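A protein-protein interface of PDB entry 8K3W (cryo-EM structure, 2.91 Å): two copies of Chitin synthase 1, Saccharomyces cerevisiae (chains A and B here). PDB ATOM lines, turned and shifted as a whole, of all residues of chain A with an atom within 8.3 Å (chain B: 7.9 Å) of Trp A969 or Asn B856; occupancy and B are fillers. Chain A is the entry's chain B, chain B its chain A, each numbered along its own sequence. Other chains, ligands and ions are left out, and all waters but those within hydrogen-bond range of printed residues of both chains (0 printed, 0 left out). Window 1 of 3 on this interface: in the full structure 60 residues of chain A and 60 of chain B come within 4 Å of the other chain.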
ATOM      1  N   LEU A 854      14.624  16.777 -10.199  1.00  0.00           N
ATOM      2  CA  LEU A 854      14.156  16.234  -8.931  1.00  0.00           C
ATOM      3  C   LEU A 854      14.204  14.712  -8.911  1.00  0.00           C
ATOM      4  O   LEU A 854      14.524  14.115  -7.879  1.00  0.00           O
ATOM      5  CB  LEU A 854      12.736  16.719  -8.644  1.00  0.00           C
ATOM      6  CG  LEU A 854      12.611  18.071  -7.950  1.00  0.00           C
ATOM      7  CD1 LEU A 854      11.224  18.638  -8.157  1.00  0.00           C
ATOM      8  CD2 LEU A 854      12.914  17.932  -6.475  1.00  0.00           C
ATOM      9  N   ASP A 966      23.299  15.647  -1.404  1.00  0.00           N
ATOM     10  CA  ASP A 966      23.151  14.332  -2.081  1.00  0.00           C
ATOM     11  C   ASP A 966      22.513  13.360  -1.082  1.00  0.00           C
ATOM     12  O   ASP A 966      23.255  12.808  -0.251  1.00  0.00           O
ATOM     13  CB  ASP A 966      24.489  13.819  -2.608  1.00  0.00           C
ATOM     14  N   LEU A 967      21.194  13.172  -1.160  1.00  0.00           N
ATOM     15  CA  LEU A 967      20.477  12.316  -0.173  1.00  0.00           C
ATOM     16  C   LEU A 967      20.493  10.855  -0.633  1.00  0.00           C
ATOM     17  O   LEU A 967      19.789  10.542  -1.611  1.00  0.00           O
ATOM     18  CB  LEU A 967      19.040  12.826  -0.031  1.00  0.00           C
ATOM     19  CG  LEU A 967      18.855  14.032   0.887  1.00  0.00           C
ATOM     20  CD1 LEU A 967      19.607  13.825   2.189  1.00  0.00           C
ATOM     21  CD2 LEU A 967      19.319  15.308   0.205  1.00  0.00           C
ATOM     22  N   SER A 968      21.262  10.000   0.048  1.00  0.00           N
ATOM     23  CA  SER A 968      21.274   8.547  -0.267  1.00  0.00           C
ATOM     24  C   SER A 968      20.464   7.830   0.809  1.00  0.00           C
ATOM     25  O   SER A 968      21.038   7.527   1.871  1.00  0.00           O
ATOM     26  CB  SER A 968      22.679   8.026  -0.334  1.00  0.00           C
ATOM     27  OG  SER A 968      23.375   8.305   0.874  1.00  0.00           O
ATOM     28  N   TRP A 969      19.180   7.568   0.552  1.00  0.00           N
ATOM     29  CA  TRP A 969      18.335   7.010   1.603  1.00  0.00           C
ATOM     30  C   TRP A 969      18.846   5.648   2.057  1.00  0.00           C
ATOM     31  O   TRP A 969      19.254   5.481   3.212  1.00  0.00           O
ATOM     32  CB  TRP A 969      16.890   6.917   1.113  1.00  0.00           C
ATOM     33  CG  TRP A 969      16.234   8.254   0.936  1.00  0.00           C
ATOM     34  CD1 TRP A 969      16.151   8.977  -0.216  1.00  0.00           C
ATOM     35  CD2 TRP A 969      15.579   9.030   1.945  1.00  0.00           C
ATOM     36  NE1 TRP A 969      15.482  10.153   0.011  1.00  0.00           N
ATOM     37  CE2 TRP A 969      15.118  10.210   1.331  1.00  0.00           C
ATOM     38  CE3 TRP A 969      15.333   8.839   3.309  1.00  0.00           C
ATOM     39  CZ2 TRP A 969      14.431  11.194   2.032  1.00  0.00           C
ATOM     40  CZ3 TRP A 969      14.649   9.819   4.000  1.00  0.00           C
ATOM     41  CH2 TRP A 969      14.205  10.980   3.363  1.00  0.00           C
ATOM     42  N   ASP A1029      21.997   8.028  11.076  1.00  0.00           N
ATOM     43  CA  ASP A1029      22.137   8.274   9.645  1.00  0.00           C
ATOM     44  C   ASP A1029      20.800   8.625   9.007  1.00  0.00           C
ATOM     45  O   ASP A1029      20.702   9.582   8.227  1.00  0.00           O
ATOM     46  CB  ASP A1029      22.736   7.051   8.958  1.00  0.00           C
ATOM     47  CG  ASP A1029      22.719   7.168   7.449  1.00  0.00           C
ATOM     48  OD1 ASP A1029      21.670   6.867   6.835  1.00  0.00           O
ATOM     49  OD2 ASP A1029      23.757   7.536   6.868  1.00  0.00           O
ATOM     50  N   GLU A1030      19.762   7.837   9.296  1.00  0.00           N
ATOM     51  CA  GLU A1030      18.466   8.118   8.689  1.00  0.00           C
ATOM     52  C   GLU A1030      17.907   9.450   9.183  1.00  0.00           C
ATOM     53  O   GLU A1030      17.247  10.168   8.424  1.00  0.00           O
ATOM     54  CB  GLU A1030      17.468   6.980   8.950  1.00  0.00           C
ATOM     55  N   LYS A1031      18.210   9.820  10.427  1.00  0.00           N
ATOM     56  CA  LYS A1031      17.763  11.108  10.950  1.00  0.00           C
ATOM     57  C   LYS A1031      18.449  12.268  10.234  1.00  0.00           C
ATOM     58  O   LYS A1031      17.791  13.247   9.846  1.00  0.00           O
ATOM     59  CB  LYS A1031      18.008  11.145  12.459  1.00  0.00           C
ATOM     60  CG  LYS A1031      17.467  12.354  13.174  1.00  0.00           C
ATOM     61  CD  LYS A1031      17.764  12.224  14.652  1.00  0.00           C
ATOM     62  CE  LYS A1031      16.825  11.191  15.267  1.00  0.00           C
ATOM     63  NZ  LYS A1031      16.933  11.101  16.745  1.00  0.00           N
ATOM     64  N   LYS A1032      19.765  12.171  10.027  1.00  0.00           N
ATOM     65  CA  LYS A1032      20.476  13.214   9.288  1.00  0.00           C
ATOM     66  C   LYS A1032      19.997  13.296   7.845  1.00  0.00           C
ATOM     67  O   LYS A1032      19.859  14.393   7.285  1.00  0.00           O
ATOM     68  CB  LYS A1032      21.981  12.954   9.353  1.00  0.00           C
ATOM     69  CG  LYS A1032      22.847  14.093   8.873  1.00  0.00           C
ATOM     70  CD  LYS A1032      24.312  13.695   8.871  1.00  0.00           C
ATOM     71  CE  LYS A1032      24.583  12.531   7.936  1.00  0.00           C
ATOM     72  NZ  LYS A1032      26.044  12.302   7.775  1.00  0.00           N
ATOM     73  N   THR A1033      19.735  12.148   7.221  1.00  0.00           N
ATOM     74  CA  THR A1033      19.221  12.134   5.857  1.00  0.00           C
ATOM     75  C   THR A1033      17.852  12.796   5.765  1.00  0.00           C
ATOM     76  O   THR A1033      17.579  13.551   4.824  1.00  0.00           O
ATOM     77  CB  THR A1033      19.159  10.696   5.354  1.00  0.00           C
ATOM     78  OG1 THR A1033      20.480  10.144   5.332  1.00  0.00           O
ATOM     79  CG2 THR A1033      18.548  10.624   3.975  1.00  0.00           C
ATOM     80  N   GLY A1034      16.972  12.515   6.726  1.00  0.00           N
ATOM     81  CA  GLY A1034      15.682  13.179   6.737  1.00  0.00           C
ATOM     82  C   GLY A1034      15.810  14.682   6.889  1.00  0.00           C
ATOM     83  O   GLY A1034      15.127  15.447   6.200  1.00  0.00           O
ATOM     84  N   TYR A1035      16.701  15.126   7.782  1.00  0.00           N
ATOM     85  CA  TYR A1035      16.912  16.561   7.941  1.00  0.00           C
ATOM     86  C   TYR A1035      17.400  17.193   6.647  1.00  0.00           C
ATOM     87  O   TYR A1035      16.934  18.272   6.254  1.00  0.00           O
ATOM     88  CB  TYR A1035      17.908  16.827   9.066  1.00  0.00           C
ATOM     89  CG  TYR A1035      18.330  18.270   9.171  1.00  0.00           C
ATOM     90  CD1 TYR A1035      17.577  19.177   9.897  1.00  0.00           C
ATOM     91  CD2 TYR A1035      19.484  18.725   8.556  1.00  0.00           C
ATOM     92  CE1 TYR A1035      17.955  20.496   9.999  1.00  0.00           C
ATOM     93  CE2 TYR A1035      19.871  20.043   8.653  1.00  0.00           C
ATOM     94  CZ  TYR A1035      19.101  20.924   9.375  1.00  0.00           C
ATOM     95  OH  TYR A1035      19.478  22.239   9.480  1.00  0.00           O
ATOM     96  N   TYR A1036      18.347  16.542   5.972  1.00  0.00           N
ATOM     97  CA  TYR A1036      18.892  17.108   4.745  1.00  0.00           C
ATOM     98  C   TYR A1036      17.826  17.195   3.663  1.00  0.00           C
ATOM     99  O   TYR A1036      17.733  18.200   2.941  1.00  0.00           O
ATOM    100  CB  TYR A1036      20.078  16.269   4.278  1.00  0.00           C
ATOM    101  CG  TYR A1036      21.345  16.525   5.064  1.00  0.00           C
ATOM    102  CD1 TYR A1036      22.482  15.760   4.855  1.00  0.00           C
ATOM    103  CD2 TYR A1036      21.398  17.523   6.023  1.00  0.00           C
ATOM    104  CE1 TYR A1036      23.633  15.987   5.575  1.00  0.00           C
ATOM    105  CE2 TYR A1036      22.544  17.757   6.747  1.00  0.00           C
ATOM    106  CZ  TYR A1036      23.659  16.988   6.521  1.00  0.00           C
ATOM    107  OH  TYR A1036      24.804  17.224   7.248  1.00  0.00           O
ATOM    108  N   ALA A1037      16.990  16.158   3.543  1.00  0.00           N
ATOM    109  CA  ALA A1037      15.920  16.192   2.552  1.00  0.00           C
ATOM    110  C   ALA A1037      14.920  17.301   2.850  1.00  0.00           C
ATOM    111  O   ALA A1037      14.462  17.999   1.937  1.00  0.00           O
ATOM    112  CB  ALA A1037      15.219  14.837   2.493  1.00  0.00           C
ATOM    113  N   ASN A1038      14.571  17.480   4.128  1.00  0.00           N
ATOM    114  CA  ASN A1038      13.657  18.556   4.494  1.00  0.00           C
ATOM    115  C   ASN A1038      14.235  19.916   4.148  1.00  0.00           C
ATOM    116  O   ASN A1038      13.523  20.790   3.637  1.00  0.00           O
ATOM    117  CB  ASN A1038      13.334  18.495   5.983  1.00  0.00           C
ATOM    118  CG  ASN A1038      12.487  17.308   6.338  1.00  0.00           C
ATOM    119  OD1 ASN A1038      11.982  16.611   5.462  1.00  0.00           O
ATOM    120  ND2 ASN A1038      12.318  17.069   7.631  1.00  0.00           N
ATOM    121  N   VAL A1039      15.521  20.120   4.430  1.00  0.00           N
ATOM    122  CA  VAL A1039      16.140  21.396   4.090  1.00  0.00           C
ATOM    123  C   VAL A1039      16.094  21.627   2.585  1.00  0.00           C
ATOM    124  O   VAL A1039      15.765  22.732   2.130  1.00  0.00           O
ATOM    125  CB  VAL A1039      17.575  21.467   4.644  1.00  0.00           C
ATOM    126  CG1 VAL A1039      18.250  22.730   4.186  1.00  0.00           C
ATOM    127  CG2 VAL A1039      17.547  21.447   6.147  1.00  0.00           C
ATOM    128  N   ARG A1040      16.392  20.585   1.801  1.00  0.00           N
ATOM    129  CA  ARG A1040      16.424  20.705   0.319  1.00  0.00           C
ATOM    130  C   ARG A1040      15.044  21.044  -0.235  1.00  0.00           C
ATOM    131  O   ARG A1040      14.985  21.823  -1.191  1.00  0.00           O
ATOM    132  CB  ARG A1040      16.864  19.392  -0.327  1.00  0.00           C
ATOM    133  CG  ARG A1040      16.838  19.434  -1.849  1.00  0.00           C
ATOM    134  CD  ARG A1040      16.652  18.080  -2.502  1.00  0.00           C
ATOM    135  NE  ARG A1040      17.845  17.251  -2.477  1.00  0.00           N
ATOM    136  CZ  ARG A1040      17.960  16.095  -3.121  1.00  0.00           C
ATOM    137  NH1 ARG A1040      16.951  15.639  -3.843  1.00  0.00           N
ATOM    138  NH2 ARG A1040      19.081  15.402  -3.047  1.00  0.00           N
ATOM    139  N   SER A1041      13.988  20.456   0.319  1.00  0.00           N
ATOM    140  CA  SER A1041      12.638  20.675  -0.180  1.00  0.00           C
ATOM    141  C   SER A1041      12.003  21.932   0.384  1.00  0.00           C
ATOM    142  O   SER A1041      11.017  22.412  -0.181  1.00  0.00           O
ATOM    143  CB  SER A1041      11.749  19.472   0.129  1.00  0.00           C
ATOM    144  OG  SER A1041      11.157  19.598   1.407  1.00  0.00           O
ATOM    145  N   LEU A1042      12.528  22.477   1.476  1.00  0.00           N
ATOM    146  CA  LEU A1042      12.063  23.784   1.913  1.00  0.00           C
ATOM    147  C   LEU A1042      12.721  24.893   1.106  1.00  0.00           C
ATOM    148  O   LEU A1042      12.055  25.870   0.732  1.00  0.00           O
ATOM    149  CB  LEU A1042      12.327  23.956   3.415  1.00  0.00           C
ATOM    150  CG  LEU A1042      11.639  25.127   4.113  1.00  0.00           C
ATOM    151  CD1 LEU A1042      11.254  24.743   5.520  1.00  0.00           C
ATOM    152  CD2 LEU A1042      12.542  26.337   4.144  1.00  0.00           C
ATOM    153  N   SER B 848       3.394  21.993  -3.165  1.00  0.00           N
ATOM    154  CA  SER B 848       4.075  21.300  -2.082  1.00  0.00           C
ATOM    155  C   SER B 848       3.852  19.799  -2.165  1.00  0.00           C
ATOM    156  O   SER B 848       4.765  19.017  -1.877  1.00  0.00           O
ATOM    157  CB  SER B 848       3.604  21.850  -0.745  1.00  0.00           C
ATOM    158  OG  SER B 848       3.569  23.263  -0.771  1.00  0.00           O
ATOM    159  N   THR B 849       2.651  19.370  -2.543  1.00  0.00           N
ATOM    160  CA  THR B 849       2.402  17.940  -2.689  1.00  0.00           C
ATOM    161  C   THR B 849       3.278  17.339  -3.780  1.00  0.00           C
ATOM    162  O   THR B 849       3.877  16.275  -3.578  1.00  0.00           O
ATOM    163  CB  THR B 849       0.930  17.685  -2.989  1.00  0.00           C
ATOM    164  OG1 THR B 849       0.124  18.391  -2.043  1.00  0.00           O
ATOM    165  CG2 THR B 849       0.630  16.208  -2.882  1.00  0.00           C
ATOM    166  N   PHE B 850       3.381  18.004  -4.935  1.00  0.00           N
ATOM    167  CA  PHE B 850       4.285  17.514  -5.972  1.00  0.00           C
ATOM    168  C   PHE B 850       5.708  17.390  -5.449  1.00  0.00           C
ATOM    169  O   PHE B 850       6.361  16.357  -5.627  1.00  0.00           O
ATOM    170  CB  PHE B 850       4.282  18.430  -7.194  1.00  0.00           C
ATOM    171  CG  PHE B 850       3.375  17.982  -8.292  1.00  0.00           C
ATOM    172  CD1 PHE B 850       2.034  17.760  -8.068  1.00  0.00           C
ATOM    173  CD2 PHE B 850       3.884  17.724  -9.546  1.00  0.00           C
ATOM    174  CE1 PHE B 850       1.216  17.341  -9.092  1.00  0.00           C
ATOM    175  CE2 PHE B 850       3.071  17.294 -10.562  1.00  0.00           C
ATOM    176  CZ  PHE B 850       1.734  17.103 -10.335  1.00  0.00           C
ATOM    177  N   ILE B 851       6.205  18.443  -4.803  1.00  0.00           N
ATOM    178  CA  ILE B 851       7.610  18.457  -4.413  1.00  0.00           C
ATOM    179  C   ILE B 851       7.892  17.396  -3.355  1.00  0.00           C
ATOM    180  O   ILE B 851       8.892  16.672  -3.437  1.00  0.00           O
ATOM    181  CB  ILE B 851       8.011  19.864  -3.945  1.00  0.00           C
ATOM    182  CG1 ILE B 851       8.287  20.744  -5.162  1.00  0.00           C
ATOM    183  CG2 ILE B 851       9.221  19.809  -3.044  1.00  0.00           C
ATOM    184  CD1 ILE B 851       8.428  22.198  -4.842  1.00  0.00           C
ATOM    185  N   LEU B 852       7.017  17.269  -2.359  1.00  0.00           N
ATOM    186  CA  LEU B 852       7.249  16.301  -1.294  1.00  0.00           C
ATOM    187  C   LEU B 852       7.069  14.873  -1.785  1.00  0.00           C
ATOM    188  O   LEU B 852       7.751  13.961  -1.306  1.00  0.00           O
ATOM    189  CB  LEU B 852       6.326  16.586  -0.119  1.00  0.00           C
ATOM    190  CG  LEU B 852       6.552  17.928   0.566  1.00  0.00           C
ATOM    191  CD1 LEU B 852       5.471  18.178   1.583  1.00  0.00           C
ATOM    192  CD2 LEU B 852       7.911  17.965   1.216  1.00  0.00           C
ATOM    193  N   SER B 853       6.150  14.645  -2.725  1.00  0.00           N
ATOM    194  CA  SER B 853       5.993  13.298  -3.258  1.00  0.00           C
ATOM    195  C   SER B 853       7.171  12.917  -4.142  1.00  0.00           C
ATOM    196  O   SER B 853       7.567  11.748  -4.183  1.00  0.00           O
ATOM    197  CB  SER B 853       4.686  13.191  -4.032  1.00  0.00           C
ATOM    198  OG  SER B 853       4.797  13.842  -5.280  1.00  0.00           O
ATOM    199  N   LEU B 854       7.743  13.886  -4.860  1.00  0.00           N
ATOM    200  CA  LEU B 854       8.873  13.584  -5.727  1.00  0.00           C
ATOM    201  C   LEU B 854      10.163  13.400  -4.938  1.00  0.00           C
ATOM    202  O   LEU B 854      10.984  12.544  -5.281  1.00  0.00           O
ATOM    203  CB  LEU B 854       9.047  14.689  -6.767  1.00  0.00           C
ATOM    204  CG  LEU B 854       8.215  14.555  -8.040  1.00  0.00           C
ATOM    205  CD1 LEU B 854       8.107  15.893  -8.736  1.00  0.00           C
ATOM    206  CD2 LEU B 854       8.828  13.524  -8.960  1.00  0.00           C
ATOM    207  N   GLY B 855      10.362  14.185  -3.881  1.00  0.00           N
ATOM    208  CA  GLY B 855      11.628  14.156  -3.176  1.00  0.00           C
ATOM    209  C   GLY B 855      11.628  13.499  -1.810  1.00  0.00           C
ATOM    210  O   GLY B 855      12.588  12.814  -1.456  1.00  0.00           O
ATOM    211  N   ASN B 856      10.569  13.695  -1.040  1.00  0.00           N
ATOM    212  CA  ASN B 856      10.532  13.284   0.353  1.00  0.00           C
ATOM    213  C   ASN B 856       9.747  11.983   0.510  1.00  0.00           C
ATOM    214  O   ASN B 856       9.377  11.328  -0.467  1.00  0.00           O
ATOM    215  CB  ASN B 856       9.942  14.407   1.202  1.00  0.00           C
ATOM    216  CG  ASN B 856      10.608  14.525   2.546  1.00  0.00           C
ATOM    217  OD1 ASN B 856      11.190  13.566   3.044  1.00  0.00           O
ATOM    218  ND2 ASN B 856      10.531  15.703   3.143  1.00  0.00           N
ATOM    219  N   LYS B 857       9.498  11.599   1.759  1.00  0.00           N
ATOM    220  CA  LYS B 857       8.729  10.419   2.116  1.00  0.00           C
ATOM    221  C   LYS B 857       7.595  10.810   3.052  1.00  0.00           C
ATOM    222  O   LYS B 857       7.746  11.723   3.869  1.00  0.00           O
ATOM    223  CB  LYS B 857       9.612   9.364   2.794  1.00  0.00           C
ATOM    224  CG  LYS B 857      10.807   8.949   1.962  1.00  0.00           C
ATOM    225  CD  LYS B 857      10.513   7.671   1.199  1.00  0.00           C
ATOM    226  CE  LYS B 857      11.629   7.333   0.232  1.00  0.00           C
ATOM    227  NZ  LYS B 857      11.091   6.857  -1.072  1.00  0.00           N
ATOM    228  N   PRO B 858       6.445  10.135   2.950  1.00  0.00           N
ATOM    229  CA  PRO B 858       5.287  10.540   3.764  1.00  0.00           C
ATOM    230  C   PRO B 858       5.519  10.454   5.258  1.00  0.00           C
ATOM    231  O   PRO B 858       4.984  11.283   6.004  1.00  0.00           O
ATOM    232  CB  PRO B 858       4.189   9.568   3.311  1.00  0.00           C
ATOM    233  CG  PRO B 858       4.637   9.070   1.995  1.00  0.00           C
ATOM    234  CD  PRO B 858       6.123   9.009   2.063  1.00  0.00           C
ATOM    235  N   LYS B 859       6.294   9.476   5.726  1.00  0.00           N
ATOM    236  CA  LYS B 859       6.517   9.338   7.161  1.00  0.00           C
ATOM    237  C   LYS B 859       7.273  10.536   7.718  1.00  0.00           C
ATOM    238  O   LYS B 859       7.064  10.930   8.869  1.00  0.00           O
ATOM    239  CB  LYS B 859       7.277   8.046   7.451  1.00  0.00           C
ATOM    240  CG  LYS B 859       6.761   6.834   6.698  1.00  0.00           C
ATOM    241  CD  LYS B 859       5.358   6.467   7.143  1.00  0.00           C
ATOM    242  CE  LYS B 859       5.354   5.912   8.554  1.00  0.00           C
ATOM    243  NZ  LYS B 859       6.285   4.762   8.705  1.00  0.00           N
ATOM    244  N   SER B 860       8.158  11.123   6.911  1.00  0.00           N
ATOM    245  CA  SER B 860       8.977  12.236   7.376  1.00  0.00           C
ATOM    246  C   SER B 860       8.132  13.464   7.686  1.00  0.00           C
ATOM    247  O   SER B 860       8.388  14.170   8.668  1.00  0.00           O
ATOM    248  CB  SER B 860      10.042  12.568   6.335  1.00  0.00           C
ATOM    249  OG  SER B 860      10.896  13.596   6.794  1.00  0.00           O
ATOM    250  N   THR B 861       7.127  13.743   6.859  1.00  0.00           N
ATOM    251  CA  THR B 861       6.281  14.925   7.005  1.00  0.00           C
ATOM    252  C   THR B 861       4.809  14.508   7.064  1.00  0.00           C
ATOM    253  O   THR B 861       4.105  14.474   6.056  1.00  0.00           O
ATOM    254  CB  THR B 861       6.566  15.924   5.867  1.00  0.00           C
ATOM    255  OG1 THR B 861       5.683  17.048   5.977  1.00  0.00           O
ATOM    256  CG2 THR B 861       6.462  15.274   4.486  1.00  0.00           C
ATOM    257  N   TYR B 865       0.913  16.781   5.662  1.00  0.00           N
ATOM    258  CA  TYR B 865      -0.134  16.066   4.939  1.00  0.00           C
ATOM    259  C   TYR B 865      -1.479  16.214   5.636  1.00  0.00           C
ATOM    260  O   TYR B 865      -2.511  16.380   4.973  1.00  0.00           O
ATOM    261  CB  TYR B 865       0.243  14.597   4.786  1.00  0.00           C
ATOM    262  CG  TYR B 865       1.209  14.347   3.657  1.00  0.00           C
ATOM    263  CD1 TYR B 865       1.178  15.123   2.512  1.00  0.00           C
ATOM    264  CD2 TYR B 865       2.159  13.345   3.743  1.00  0.00           C
ATOM    265  CE1 TYR B 865       2.060  14.901   1.478  1.00  0.00           C
ATOM    266  CE2 TYR B 865       3.046  13.120   2.714  1.00  0.00           C
ATOM    267  CZ  TYR B 865       2.992  13.902   1.584  1.00  0.00           C
ATOM    268  OH  TYR B 865       3.875  13.674   0.558  1.00  0.00           O
ATOM    269  N   TYR B 959       0.713  11.410  -5.328  1.00  0.00           N
ATOM    270  CA  TYR B 959       1.733  10.520  -4.795  1.00  0.00           C
ATOM    271  C   TYR B 959       1.817   9.224  -5.585  1.00  0.00           C
ATOM    272  O   TYR B 959       2.912   8.693  -5.785  1.00  0.00           O
ATOM    273  CB  TYR B 959       1.464  10.223  -3.322  1.00  0.00           C
ATOM    274  CG  TYR B 959       2.583   9.458  -2.660  1.00  0.00           C
ATOM    275  CD1 TYR B 959       2.596   8.073  -2.654  1.00  0.00           C
ATOM    276  CD2 TYR B 959       3.632  10.120  -2.053  1.00  0.00           C
ATOM    277  CE1 TYR B 959       3.618   7.377  -2.060  1.00  0.00           C
ATOM    278  CE2 TYR B 959       4.658   9.432  -1.458  1.00  0.00           C
ATOM    279  CZ  TYR B 959       4.646   8.060  -1.465  1.00  0.00           C
ATOM    280  OH  TYR B 959       5.672   7.367  -0.867  1.00  0.00           O
ATOM    281  N   ASN B 963       5.376   8.202  -7.758  1.00  0.00           N
ATOM    282  CA  ASN B 963       6.102   7.056  -7.218  1.00  0.00           C
ATOM    283  C   ASN B 963       5.678   5.787  -7.933  1.00  0.00           C
ATOM    284  O   ASN B 963       5.330   4.779  -7.314  1.00  0.00           O
ATOM    285  CB  ASN B 963       5.881   6.936  -5.720  1.00  0.00           C
ATOM    286  CG  ASN B 963       6.433   8.110  -4.964  1.00  0.00           C
ATOM    287  OD1 ASN B 963       5.825   9.174  -4.928  1.00  0.00           O
ATOM    288  ND2 ASN B 963       7.594   7.928  -4.354  1.00  0.00           N
ATOM    289  N   LEU B 967      12.295   3.313  -7.176  1.00  0.00           N
ATOM    290  CA  LEU B 967      13.661   3.341  -7.770  1.00  0.00           C
ATOM    291  C   LEU B 967      14.716   3.438  -6.664  1.00  0.00           C
ATOM    292  O   LEU B 967      14.820   4.515  -6.048  1.00  0.00           O
ATOM    293  CB  LEU B 967      13.759   4.538  -8.721  1.00  0.00           C
ATOM    294  CG  LEU B 967      13.163   4.327 -10.111  1.00  0.00           C
ATOM    295  CD1 LEU B 967      13.618   2.996 -10.685  1.00  0.00           C
ATOM    296  CD2 LEU B 967      11.646   4.394 -10.066  1.00  0.00           C
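Asn B856 touches Trp A969. Ser A1041 touches Leu B852.
Positions printed for both chains: 854 and 967. Of the 4 pairs that touch across the chains among the printed residues, none has its exchanged pair printed and touching as well.
The side-chain hydroxyl (OG) of Ser B860 lies within hydrogen-bond range of the side-chain amide oxygen (OD1) of Asn A1038, 3.5 Å away. The side-chain amide oxygen (OD1) of Asn A1038 is in hydrogen-bond range of the side-chain amide nitrogen (ND2) of Asn B856 (2.9 Å).
The backbone carbonyl oxygen (O) of Asn A1038 is in hydrogen-bond range of the side-chain hydroxyl (OG) of Ser A1041 (3.5 Å). The backbone carbonyl oxygen of Gly A1034 lies close to the side-chain amide oxygen of Asn A1038 (3.4 Å).
Among the printed residues, no Asp or Glu carboxylate lies within 4 Å of a Lys or Arg side-chain nitrogen of the other chain.
Of the printed residues of chain B, Trp A969 touches Asn B856. Of the printed residues of chain A, Asn B856 touches Trp A969 and Asn A1038. No residue of chain A comes within 4 Å of Gly B855. Printed residues of chain A within 4 Å of Ser B860: Asn A1038 (3.5 Å). Printed residues of chain B within 4 Å of Asn A1038: Asn B856 (2.9 Å) and Ser B860 (3.5 Å). Of the printed residues of chain A, Leu B852 touches Ser A1041. Of the printed residues of chain B, Ser A1041 touches Leu B852 (3.6 Å). Thr B849 touches none of the printed residues of chain A. Asp A1029 touches none of the printed residues of chain B. The nearest printed residue of chain A that does not touch Asn B856 is Ala A1037 (4.3 Å).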
